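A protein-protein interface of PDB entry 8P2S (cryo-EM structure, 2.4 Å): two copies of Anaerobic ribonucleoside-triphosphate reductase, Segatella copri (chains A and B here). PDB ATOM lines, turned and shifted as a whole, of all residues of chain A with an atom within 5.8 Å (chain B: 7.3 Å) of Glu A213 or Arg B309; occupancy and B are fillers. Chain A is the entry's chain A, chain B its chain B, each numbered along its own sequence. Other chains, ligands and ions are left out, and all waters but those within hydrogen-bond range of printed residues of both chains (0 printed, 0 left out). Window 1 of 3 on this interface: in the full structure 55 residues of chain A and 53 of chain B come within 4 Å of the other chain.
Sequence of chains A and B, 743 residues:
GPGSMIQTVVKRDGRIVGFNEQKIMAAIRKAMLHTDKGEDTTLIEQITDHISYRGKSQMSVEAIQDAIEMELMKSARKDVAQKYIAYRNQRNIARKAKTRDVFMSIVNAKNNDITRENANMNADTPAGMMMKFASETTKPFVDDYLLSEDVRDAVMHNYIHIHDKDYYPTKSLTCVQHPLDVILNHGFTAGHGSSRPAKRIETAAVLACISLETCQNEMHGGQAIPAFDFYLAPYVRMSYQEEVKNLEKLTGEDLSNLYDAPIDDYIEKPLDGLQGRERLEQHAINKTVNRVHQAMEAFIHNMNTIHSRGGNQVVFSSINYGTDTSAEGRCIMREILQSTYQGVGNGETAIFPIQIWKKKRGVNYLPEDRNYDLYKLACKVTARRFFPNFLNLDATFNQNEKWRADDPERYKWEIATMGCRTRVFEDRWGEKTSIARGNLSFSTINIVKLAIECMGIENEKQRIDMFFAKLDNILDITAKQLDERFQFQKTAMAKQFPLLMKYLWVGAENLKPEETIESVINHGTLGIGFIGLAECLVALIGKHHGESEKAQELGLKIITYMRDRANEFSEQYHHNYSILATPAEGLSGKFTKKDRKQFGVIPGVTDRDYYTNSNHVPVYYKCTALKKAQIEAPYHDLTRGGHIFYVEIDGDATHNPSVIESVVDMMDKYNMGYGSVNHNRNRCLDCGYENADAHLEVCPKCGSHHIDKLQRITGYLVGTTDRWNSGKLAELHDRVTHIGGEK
NH2 of Arg B309 is in salt-bridge range of OE1 of Glu A213, at 3.1 Å.
OG of Ser A308 sits close to NH2 of Arg B309, 3.3 Å away.
N of Ala B127 sits at hydrogen-bond distance from O of Asn A217, at 3.4 Å.
The side-chain amide nitrogen (ND2) of Asn A217 lies close to the backbone NH (N) of Gly B311, at 3.0 Å.
The guanidinium group (NH2) of Arg B309 lies within salt-bridge range of the side-chain carboxylate (OE2) of Glu B213 (3.3 Å).
The backbone carbonyl oxygen (O) of Ile A210 is in hydrogen-bond range of the side-chain hydroxyl (OG1) of Thr A214, at 2.7 Å.
The side-chain amide oxygen (OD1) of Asn B217 sits close to the side-chain amide oxygen (OD1) of Asn B312 (2.9 Å).
OG of Ser B308 lies within hydrogen-bond range of O of Thr B305 (2.6 Å).
Among the printed residues, merely in contact across the chains: Ile A210 with Thr B305, Thr A214 with Arg B309, Asn A217 with Arg B309, Asn A217 with Gly B310, Ser A308 with Gly B311 and Ser A308 with Asn B312.
Of chain B, only Arg B309 comes within 4 Å of Glu A213.
Arg B309 touches four residues of chain A.
Of the printed residues of chain B, Asn A217 touches Ala B127 (3.4 Å), Arg B309 (3.3 Å), Gly B310 (3.4 Å) and Gly B311 (3.0 Å).
Of the printed residues of chain B, Ser A308 touches Arg B309 (3.1 Å), Gly B311 (3.8 Å) and Asn B312 (3.5 Å).
Asn B302 touches none of the printed residues of chain A.
Asn B304 touches none of the printed residues of chain A.
The nearest residue of chain B that does not touch Glu A213 is Ile B306 (4.7 Å).
The nearest residue of chain A that does not touch Arg B309 is Ile A306 (4.9 Å).
Of the 18 printed residues of chain A, 5 touch a printed residue of chain B.
Hydrophobic or aromatic side chains of chain A that line the printed part of chain B: Ile A210.
Of the 19 printed residues of chain B, 6 touch a printed residue of chain A.
Hydrophobic or aromatic side chains of chain B that line the printed part of chain A: Ala B127.
Along chain B the printed residues that touch a printed residue of chain A span positions 127 to 312.
Among the printed residues, Asp or Glu carboxylates within 4 Å of a Lys or Arg side-chain nitrogen of the other chain: Glu A213 with Arg B309 (3.1 Å).
6 positions are printed for both chains.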
ATOM      1  N   HIS A 178       0.602  23.789  31.072  1.00  0.00           N
ATOM      2  CA  HIS A 178       1.798  22.970  31.161  1.00  0.00           C
ATOM      3  C   HIS A 178       1.984  22.425  32.569  1.00  0.00           C
ATOM      4  O   HIS A 178       2.028  23.211  33.528  1.00  0.00           O
ATOM      5  CB  HIS A 178       3.025  23.790  30.773  1.00  0.00           C
ATOM      6  CG  HIS A 178       3.010  24.277  29.360  1.00  0.00           C
ATOM      7  ND1 HIS A 178       4.050  24.052  28.488  1.00  0.00           N
ATOM      8  CD2 HIS A 178       2.084  24.983  28.670  1.00  0.00           C
ATOM      9  CE1 HIS A 178       3.767  24.598  27.319  1.00  0.00           C
ATOM     10  NE2 HIS A 178       2.578  25.167  27.402  1.00  0.00           N
ATOM     11  N   ALA A 208      10.958  27.000  31.856  1.00  0.00           N
ATOM     12  CA  ALA A 208       9.556  27.362  31.662  1.00  0.00           C
ATOM     13  C   ALA A 208       9.357  28.063  30.323  1.00  0.00           C
ATOM     14  O   ALA A 208       8.435  27.734  29.560  1.00  0.00           O
ATOM     15  CB  ALA A 208       9.081  28.249  32.812  1.00  0.00           C
ATOM     16  N   CYS A 209      10.232  29.025  30.014  1.00  0.00           N
ATOM     17  CA  CYS A 209      10.164  29.702  28.722  1.00  0.00           C
ATOM     18  C   CYS A 209      10.335  28.714  27.576  1.00  0.00           C
ATOM     19  O   CYS A 209       9.621  28.787  26.569  1.00  0.00           O
ATOM     20  CB  CYS A 209      11.231  30.794  28.637  1.00  0.00           C
ATOM     21  SG  CYS A 209      11.061  32.134  29.825  1.00  0.00           S
ATOM     22  N   ILE A 210      11.281  27.784  27.715  1.00  0.00           N
ATOM     23  CA  ILE A 210      11.551  26.808  26.666  1.00  0.00           C
ATOM     24  C   ILE A 210      10.347  25.904  26.452  1.00  0.00           C
ATOM     25  O   ILE A 210       9.977  25.605  25.313  1.00  0.00           O
ATOM     26  CB  ILE A 210      12.815  25.997  27.010  1.00  0.00           C
ATOM     27  CG1 ILE A 210      14.074  26.830  26.760  1.00  0.00           C
ATOM     28  CG2 ILE A 210      12.853  24.704  26.222  1.00  0.00           C
ATOM     29  CD1 ILE A 210      14.229  27.287  25.325  1.00  0.00           C
ATOM     30  N   SER A 211       9.726  25.443  27.539  1.00  0.00           N
ATOM     31  CA  SER A 211       8.548  24.592  27.417  1.00  0.00           C
ATOM     32  C   SER A 211       7.417  25.327  26.713  1.00  0.00           C
ATOM     33  O   SER A 211       6.775  24.783  25.804  1.00  0.00           O
ATOM     34  CB  SER A 211       8.103  24.113  28.798  1.00  0.00           C
ATOM     35  OG  SER A 211       6.943  23.307  28.708  1.00  0.00           O
ATOM     36  N   LEU A 212       7.168  26.578  27.111  1.00  0.00           N
ATOM     37  CA  LEU A 212       6.101  27.349  26.480  1.00  0.00           C
ATOM     38  C   LEU A 212       6.377  27.558  24.996  1.00  0.00           C
ATOM     39  O   LEU A 212       5.486  27.382  24.156  1.00  0.00           O
ATOM     40  CB  LEU A 212       5.928  28.689  27.194  1.00  0.00           C
ATOM     41  CG  LEU A 212       5.466  28.627  28.650  1.00  0.00           C
ATOM     42  CD1 LEU A 212       5.302  30.022  29.224  1.00  0.00           C
ATOM     43  CD2 LEU A 212       4.174  27.845  28.771  1.00  0.00           C
ATOM     44  N   GLU A 213       7.615  27.921  24.650  1.00  0.00           N
ATOM     45  CA  GLU A 213       7.954  28.165  23.251  1.00  0.00           C
ATOM     46  C   GLU A 213       7.881  26.887  22.424  1.00  0.00           C
ATOM     47  O   GLU A 213       7.396  26.905  21.287  1.00  0.00           O
ATOM     48  CB  GLU A 213       9.344  28.788  23.150  1.00  0.00           C
ATOM     49  CG  GLU A 213       9.439  30.186  23.736  1.00  0.00           C
ATOM     50  CD  GLU A 213      10.861  30.707  23.769  1.00  0.00           C
ATOM     51  OE1 GLU A 213      11.736  30.093  23.123  1.00  0.00           O
ATOM     52  OE2 GLU A 213      11.106  31.728  24.445  1.00  0.00           O
ATOM     53  N   THR A 214       8.365  25.770  22.974  1.00  0.00           N
ATOM     54  CA  THR A 214       8.345  24.508  22.245  1.00  0.00           C
ATOM     55  C   THR A 214       6.921  24.033  22.004  1.00  0.00           C
ATOM     56  O   THR A 214       6.587  23.584  20.901  1.00  0.00           O
ATOM     57  CB  THR A 214       9.137  23.450  23.010  1.00  0.00           C
ATOM     58  OG1 THR A 214      10.471  23.920  23.235  1.00  0.00           O
ATOM     59  CG2 THR A 214       9.191  22.152  22.225  1.00  0.00           C
ATOM     60  N   CYS A 215       6.060  24.128  23.019  1.00  0.00           N
ATOM     61  CA  CYS A 215       4.684  23.689  22.845  1.00  0.00           C
ATOM     62  C   CYS A 215       3.850  24.684  22.050  1.00  0.00           C
ATOM     63  O   CYS A 215       2.782  24.314  21.550  1.00  0.00           O
ATOM     64  CB  CYS A 215       4.041  23.431  24.207  1.00  0.00           C
ATOM     65  SG  CYS A 215       2.519  22.465  24.150  1.00  0.00           S
ATOM     66  N   GLN A 216       4.307  25.931  21.919  1.00  0.00           N
ATOM     67  CA  GLN A 216       3.598  26.885  21.075  1.00  0.00           C
ATOM     68  C   GLN A 216       3.778  26.564  19.597  1.00  0.00           C
ATOM     69  O   GLN A 216       2.924  26.916  18.778  1.00  0.00           O
ATOM     70  CB  GLN A 216       4.070  28.307  21.375  1.00  0.00           C
ATOM     71  CG  GLN A 216       3.323  29.395  20.618  1.00  0.00           C
ATOM     72  CD  GLN A 216       1.863  29.491  21.014  1.00  0.00           C
ATOM     73  OE1 GLN A 216       1.517  30.155  21.989  1.00  0.00           O
ATOM     74  NE2 GLN A 216       0.998  28.828  20.256  1.00  0.00           N
ATOM     75  N   ASN A 217       4.876  25.905  19.236  1.00  0.00           N
ATOM     76  CA  ASN A 217       5.086  25.476  17.860  1.00  0.00           C
ATOM     77  C   ASN A 217       4.398  24.157  17.544  1.00  0.00           C
ATOM     78  O   ASN A 217       4.426  23.721  16.389  1.00  0.00           O
ATOM     79  CB  ASN A 217       6.583  25.367  17.566  1.00  0.00           C
ATOM     80  CG  ASN A 217       7.292  26.697  17.670  1.00  0.00           C
ATOM     81  OD1 ASN A 217       6.677  27.753  17.530  1.00  0.00           O
ATOM     82  ND2 ASN A 217       8.596  26.657  17.910  1.00  0.00           N
ATOM     83  N   GLU A 218       3.792  23.512  18.537  1.00  0.00           N
ATOM     84  CA  GLU A 218       3.027  22.293  18.334  1.00  0.00           C
ATOM     85  C   GLU A 218       1.527  22.518  18.454  1.00  0.00           C
ATOM     86  O   GLU A 218       0.751  21.604  18.161  1.00  0.00           O
ATOM     87  CB  GLU A 218       3.468  21.225  19.336  1.00  0.00           C
ATOM     88  CG  GLU A 218       4.965  21.003  19.376  1.00  0.00           C
ATOM     89  CD  GLU A 218       5.382  20.066  20.488  1.00  0.00           C
ATOM     90  OE1 GLU A 218       4.495  19.426  21.091  1.00  0.00           O
ATOM     91  OE2 GLU A 218       6.595  19.972  20.764  1.00  0.00           O
ATOM     92  N   GLN A 223      -0.539  29.108  25.713  1.00  0.00           N
ATOM     93  CA  GLN A 223       0.192  28.246  26.630  1.00  0.00           C
ATOM     94  C   GLN A 223       0.114  28.851  28.022  1.00  0.00           C
ATOM     95  O   GLN A 223       0.365  30.051  28.190  1.00  0.00           O
ATOM     96  CB  GLN A 223       1.654  28.104  26.201  1.00  0.00           C
ATOM     97  CG  GLN A 223       1.853  27.832  24.726  1.00  0.00           C
ATOM     98  CD  GLN A 223       1.337  26.476  24.313  1.00  0.00           C
ATOM     99  OE1 GLN A 223       1.272  25.552  25.120  1.00  0.00           O
ATOM    100  NE2 GLN A 223       0.964  26.348  23.046  1.00  0.00           N
ATOM    101  N   ASN A 302      11.883  37.497  28.390  1.00  0.00           N
ATOM    102  CA  ASN A 302      11.920  36.447  27.382  1.00  0.00           C
ATOM    103  C   ASN A 302      10.541  36.201  26.789  1.00  0.00           C
ATOM    104  O   ASN A 302      10.411  36.001  25.576  1.00  0.00           O
ATOM    105  CB  ASN A 302      12.484  35.163  27.983  1.00  0.00           C
ATOM    106  CG  ASN A 302      13.962  35.263  28.287  1.00  0.00           C
ATOM    107  OD1 ASN A 302      14.686  36.031  27.653  1.00  0.00           O
ATOM    108  ND2 ASN A 302      14.421  34.485  29.258  1.00  0.00           N
ATOM    109  N   MET A 303       9.498  36.208  27.621  1.00  0.00           N
ATOM    110  CA  MET A 303       8.160  36.000  27.083  1.00  0.00           C
ATOM    111  C   MET A 303       7.636  37.224  26.345  1.00  0.00           C
ATOM    112  O   MET A 303       6.734  37.089  25.513  1.00  0.00           O
ATOM    113  CB  MET A 303       7.192  35.604  28.199  1.00  0.00           C
ATOM    114  CG  MET A 303       7.596  34.350  28.954  1.00  0.00           C
ATOM    115  SD  MET A 303       8.197  33.018  27.897  1.00  0.00           S
ATOM    116  CE  MET A 303       6.740  32.630  26.938  1.00  0.00           C
ATOM    117  N   ILE A 306      11.194  37.355  23.007  1.00  0.00           N
ATOM    118  CA  ILE A 306      11.459  36.264  22.077  1.00  0.00           C
ATOM    119  C   ILE A 306      10.250  36.073  21.175  1.00  0.00           C
ATOM    120  O   ILE A 306       9.134  35.821  21.645  1.00  0.00           O
ATOM    121  CB  ILE A 306      11.810  34.978  22.827  1.00  0.00           C
ATOM    122  CG1 ILE A 306      13.262  35.020  23.303  1.00  0.00           C
ATOM    123  CG2 ILE A 306      11.586  33.766  21.936  1.00  0.00           C
ATOM    124  CD1 ILE A 306      14.265  34.980  22.172  1.00  0.00           C
ATOM    125  N   SER A 308       8.943  33.645  18.839  1.00  0.00           N
ATOM    126  CA  SER A 308       9.246  32.238  18.608  1.00  0.00           C
ATOM    127  C   SER A 308       8.281  31.553  17.653  1.00  0.00           C
ATOM    128  O   SER A 308       8.719  30.849  16.737  1.00  0.00           O
ATOM    129  CB  SER A 308       9.269  31.489  19.947  1.00  0.00           C
ATOM    130  OG  SER A 308       9.597  30.123  19.763  1.00  0.00           O
ATOM    131  N   VAL A 315       4.682  34.476  21.565  1.00  0.00           N
ATOM    132  CA  VAL A 315       4.010  33.332  22.167  1.00  0.00           C
ATOM    133  C   VAL A 315       2.853  33.804  23.037  1.00  0.00           C
ATOM    134  O   VAL A 315       2.979  34.769  23.803  1.00  0.00           O
ATOM    135  CB  VAL A 315       5.014  32.494  22.977  1.00  0.00           C
ATOM    136  CG1 VAL A 315       4.326  31.311  23.630  1.00  0.00           C
ATOM    137  CG2 VAL A 315       6.148  32.023  22.085  1.00  0.00           C
ATOM    138  N   ASN B 120      17.102  19.879   8.976  1.00  0.00           N
ATOM    139  CA  ASN B 120      16.928  20.568  10.248  1.00  0.00           C
ATOM    140  C   ASN B 120      15.465  20.745  10.624  1.00  0.00           C
ATOM    141  O   ASN B 120      15.122  20.665  11.809  1.00  0.00           O
ATOM    142  CB  ASN B 120      17.608  21.938  10.208  1.00  0.00           C
ATOM    143  CG  ASN B 120      19.116  21.844  10.295  1.00  0.00           C
ATOM    144  OD1 ASN B 120      19.656  20.947  10.943  1.00  0.00           O
ATOM    145  ND2 ASN B 120      19.805  22.775   9.647  1.00  0.00           N
ATOM    146  N   MET B 121      14.598  20.982   9.644  1.00  0.00           N
ATOM    147  CA  MET B 121      13.180  21.173   9.911  1.00  0.00           C
ATOM    148  C   MET B 121      12.500  19.822  10.080  1.00  0.00           C
ATOM    149  O   MET B 121      12.677  18.923   9.254  1.00  0.00           O
ATOM    150  CB  MET B 121      12.525  21.959   8.775  1.00  0.00           C
ATOM    151  CG  MET B 121      11.069  22.336   9.017  1.00  0.00           C
ATOM    152  SD  MET B 121      10.847  23.682  10.201  1.00  0.00           S
ATOM    153  CE  MET B 121      10.541  22.784  11.721  1.00  0.00           C
ATOM    154  N   THR B 125       6.045  17.944  12.762  1.00  0.00           N
ATOM    155  CA  THR B 125       5.481  18.940  13.656  1.00  0.00           C
ATOM    156  C   THR B 125       4.553  19.881  12.903  1.00  0.00           C
ATOM    157  O   THR B 125       4.697  20.078  11.692  1.00  0.00           O
ATOM    158  CB  THR B 125       6.597  19.738  14.325  1.00  0.00           C
ATOM    159  OG1 THR B 125       7.315  20.483  13.333  1.00  0.00           O
ATOM    160  CG2 THR B 125       7.558  18.804  15.039  1.00  0.00           C
ATOM    161  N   ALA B 127       4.508  23.106  13.007  1.00  0.00           N
ATOM    162  CA  ALA B 127       5.314  24.180  12.437  1.00  0.00           C
ATOM    163  C   ALA B 127       6.027  23.719  11.173  1.00  0.00           C
ATOM    164  O   ALA B 127       6.108  24.463  10.188  1.00  0.00           O
ATOM    165  CB  ALA B 127       6.315  24.689  13.472  1.00  0.00           C
ATOM    166  N   GLU B 213      18.114  34.150  17.580  1.00  0.00           N
ATOM    167  CA  GLU B 213      16.746  33.750  17.257  1.00  0.00           C
ATOM    168  C   GLU B 213      16.014  34.840  16.476  1.00  0.00           C
ATOM    169  O   GLU B 213      15.332  34.557  15.480  1.00  0.00           O
ATOM    170  CB  GLU B 213      15.989  33.411  18.541  1.00  0.00           C
ATOM    171  CG  GLU B 213      14.511  33.119  18.345  1.00  0.00           C
ATOM    172  CD  GLU B 213      14.224  31.641  18.189  1.00  0.00           C
ATOM    173  OE1 GLU B 213      15.124  30.829  18.485  1.00  0.00           O
ATOM    174  OE2 GLU B 213      13.099  31.291  17.774  1.00  0.00           O
ATOM    175  N   ASN B 217      14.607  34.700  12.604  1.00  0.00           N
ATOM    176  CA  ASN B 217      13.238  34.978  12.196  1.00  0.00           C
ATOM    177  C   ASN B 217      13.152  35.998  11.064  1.00  0.00           C
ATOM    178  O   ASN B 217      12.070  36.178  10.496  1.00  0.00           O
ATOM    179  CB  ASN B 217      12.418  35.466  13.391  1.00  0.00           C
ATOM    180  CG  ASN B 217      12.255  34.403  14.454  1.00  0.00           C
ATOM    181  OD1 ASN B 217      12.363  33.210  14.175  1.00  0.00           O
ATOM    182  ND2 ASN B 217      11.991  34.831  15.682  1.00  0.00           N
ATOM    183  N   ASN B 302      20.715  26.151  24.737  1.00  0.00           N
ATOM    184  CA  ASN B 302      19.663  26.937  24.107  1.00  0.00           C
ATOM    185  C   ASN B 302      19.718  26.825  22.591  1.00  0.00           C
ATOM    186  O   ASN B 302      18.685  26.589  21.954  1.00  0.00           O
ATOM    187  CB  ASN B 302      19.760  28.398  24.541  1.00  0.00           C
ATOM    188  CG  ASN B 302      19.318  28.607  25.974  1.00  0.00           C
ATOM    189  OD1 ASN B 302      18.558  27.813  26.524  1.00  0.00           O
ATOM    190  ND2 ASN B 302      19.789  29.687  26.589  1.00  0.00           N
ATOM    191  N   ASN B 304      20.853  24.382  20.990  1.00  0.00           N
ATOM    192  CA  ASN B 304      20.450  23.027  20.657  1.00  0.00           C
ATOM    193  C   ASN B 304      18.971  22.785  20.913  1.00  0.00           C
ATOM    194  O   ASN B 304      18.438  21.761  20.476  1.00  0.00           O
ATOM    195  CB  ASN B 304      21.289  22.017  21.448  1.00  0.00           C
ATOM    196  CG  ASN B 304      21.071  20.590  20.992  1.00  0.00           C
ATOM    197  OD1 ASN B 304      21.621  20.157  19.983  1.00  0.00           O
ATOM    198  ND2 ASN B 304      20.266  19.848  21.741  1.00  0.00           N
ATOM    199  N   THR B 305      18.295  23.710  21.591  1.00  0.00           N
ATOM    200  CA  THR B 305      16.869  23.583  21.859  1.00  0.00           C
ATOM    201  C   THR B 305      16.021  24.477  20.968  1.00  0.00           C
ATOM    202  O   THR B 305      15.079  23.991  20.334  1.00  0.00           O
ATOM    203  CB  THR B 305      16.572  23.900  23.327  1.00  0.00           C
ATOM    204  OG1 THR B 305      17.333  23.025  24.168  1.00  0.00           O
ATOM    205  CG2 THR B 305      15.099  23.702  23.617  1.00  0.00           C
ATOM    206  N   ILE B 306      16.345  25.769  20.882  1.00  0.00           N
ATOM    207  CA  ILE B 306      15.621  26.664  19.986  1.00  0.00           C
ATOM    208  C   ILE B 306      15.845  26.321  18.524  1.00  0.00           C
ATOM    209  O   ILE B 306      15.218  26.930  17.650  1.00  0.00           O
ATOM    210  CB  ILE B 306      16.006  28.135  20.237  1.00  0.00           C
ATOM    211  CG1 ILE B 306      17.406  28.427  19.700  1.00  0.00           C
ATOM    212  CG2 ILE B 306      15.919  28.461  21.723  1.00  0.00           C
ATOM    213  CD1 ILE B 306      17.871  29.843  19.964  1.00  0.00           C
ATOM    214  N   HIS B 307      16.740  25.376  18.233  1.00  0.00           N
ATOM    215  CA  HIS B 307      16.837  24.783  16.907  1.00  0.00           C
ATOM    216  C   HIS B 307      16.020  23.503  16.800  1.00  0.00           C
ATOM    217  O   HIS B 307      15.432  23.231  15.746  1.00  0.00           O
ATOM    218  CB  HIS B 307      18.298  24.494  16.555  1.00  0.00           C
ATOM    219  CG  HIS B 307      18.464  23.669  15.317  1.00  0.00           C
ATOM    220  ND1 HIS B 307      18.584  22.297  15.350  1.00  0.00           N
ATOM    221  CD2 HIS B 307      18.524  24.020  14.011  1.00  0.00           C
ATOM    222  CE1 HIS B 307      18.715  21.838  14.118  1.00  0.00           C
ATOM    223  NE2 HIS B 307      18.682  22.864  13.286  1.00  0.00           N
ATOM    224  N   SER B 308      15.973  22.706  17.872  1.00  0.00           N
ATOM    225  CA  SER B 308      15.156  21.497  17.854  1.00  0.00           C
ATOM    226  C   SER B 308      13.680  21.834  17.716  1.00  0.00           C
ATOM    227  O   SER B 308      12.900  21.019  17.211  1.00  0.00           O
ATOM    228  CB  SER B 308      15.399  20.672  19.116  1.00  0.00           C
ATOM    229  OG  SER B 308      15.002  21.384  20.274  1.00  0.00           O
ATOM    230  N   ARG B 309      13.279  23.021  18.157  1.00  0.00           N
ATOM    231  CA  ARG B 309      11.927  23.524  17.971  1.00  0.00           C
ATOM    232  C   ARG B 309      12.008  24.813  17.164  1.00  0.00           C
ATOM    233  O   ARG B 309      12.799  25.704  17.488  1.00  0.00           O
ATOM    234  CB  ARG B 309      11.233  23.751  19.317  1.00  0.00           C
ATOM    235  CG  ARG B 309      11.834  24.854  20.178  1.00  0.00           C
ATOM    236  CD  ARG B 309      10.942  26.085  20.170  1.00  0.00           C
ATOM    237  NE  ARG B 309      11.633  27.286  20.623  1.00  0.00           N
ATOM    238  CZ  ARG B 309      12.104  28.225  19.815  1.00  0.00           C
ATOM    239  NH1 ARG B 309      11.979  28.135  18.501  1.00  0.00           N
ATOM    240  NH2 ARG B 309      12.714  29.286  20.339  1.00  0.00           N
ATOM    241  N   GLY B 310      11.223  24.896  16.098  1.00  0.00           N
ATOM    242  CA  GLY B 310      11.168  26.123  15.335  1.00  0.00           C
ATOM    243  C   GLY B 310       9.809  26.370  14.720  1.00  0.00           C
ATOM    244  O   GLY B 310       9.314  25.547  13.946  1.00  0.00           O
ATOM    245  N   GLY B 311       9.201  27.507  15.046  1.00  0.00           N
ATOM    246  CA  GLY B 311       7.951  27.891  14.425  1.00  0.00           C
ATOM    247  C   GLY B 311       8.231  28.596  13.119  1.00  0.00           C
ATOM    248  O   GLY B 311       7.565  28.361  12.105  1.00  0.00           O
ATOM    249  N   ASN B 312       9.228  29.470  13.143  1.00  0.00           N
ATOM    250  CA  ASN B 312       9.770  30.079  11.942  1.00  0.00           C
ATOM    251  C   ASN B 312      10.892  29.187  11.417  1.00  0.00           C
ATOM    252  O   ASN B 312      10.960  27.994  11.728  1.00  0.00           O
ATOM    253  CB  ASN B 312      10.232  31.502  12.239  1.00  0.00           C
ATOM    254  CG  ASN B 312       9.196  32.296  13.005  1.00  0.00           C
ATOM    255  OD1 ASN B 312       9.506  32.947  14.003  1.00  0.00           O
ATOM    256  ND2 ASN B 312       7.954  32.238  12.548  1.00  0.00           N
ATOM    257  N   GLN B 313      11.770  29.745  10.587  1.00  0.00           N
ATOM    258  CA  GLN B 313      12.908  28.979  10.097  1.00  0.00           C
ATOM    259  C   GLN B 313      13.772  28.504  11.260  1.00  0.00           C
ATOM    260  O   GLN B 313      13.983  29.230  12.235  1.00  0.00           O
ATOM    261  CB  GLN B 313      13.738  29.819   9.129  1.00  0.00           C
ATOM    262  CG  GLN B 313      14.839  29.036   8.440  1.00  0.00           C
ATOM    263  CD  GLN B 313      15.039  29.474   7.011  1.00  0.00           C
ATOM    264  OE1 GLN B 313      14.441  30.451   6.567  1.00  0.00           O
ATOM    265  NE2 GLN B 313      15.876  28.752   6.278  1.00  0.00           N
ATOM    266  N   VAL B 314      14.257  27.265  11.154  1.00  0.00           N
ATOM    267  CA  VAL B 314      15.063  26.686  12.221  1.00  0.00           C
ATOM    268  C   VAL B 314      16.303  27.541  12.471  1.00  0.00           C
ATOM    269  O   VAL B 314      16.831  28.207  11.573  1.00  0.00           O
ATOM    270  CB  VAL B 314      15.453  25.238  11.883  1.00  0.00           C
ATOM    271  CG1 VAL B 314      14.234  24.334  11.944  1.00  0.00           C
ATOM    272  CG2 VAL B 314      16.081  25.180  10.507  1.00  0.00           C
ATOM    273  N   VAL B 315      16.770  27.515  13.719  1.00  0.00           N
ATOM    274  CA  VAL B 315      17.865  28.383  14.156  1.00  0.00           C
ATOM    275  C   VAL B 315      19.166  27.658  13.828  1.00  0.00           C
ATOM    276  O   VAL B 315      19.650  26.818  14.585  1.00  0.00           O
ATOM    277  CB  VAL B 315      17.756  28.744  15.633  1.00  0.00           C
ATOM    278  CG1 VAL B 315      18.892  29.668  16.034  1.00  0.00           C
ATOM    279  CG2 VAL B 315      16.415  29.398  15.913  1.00  0.00           C
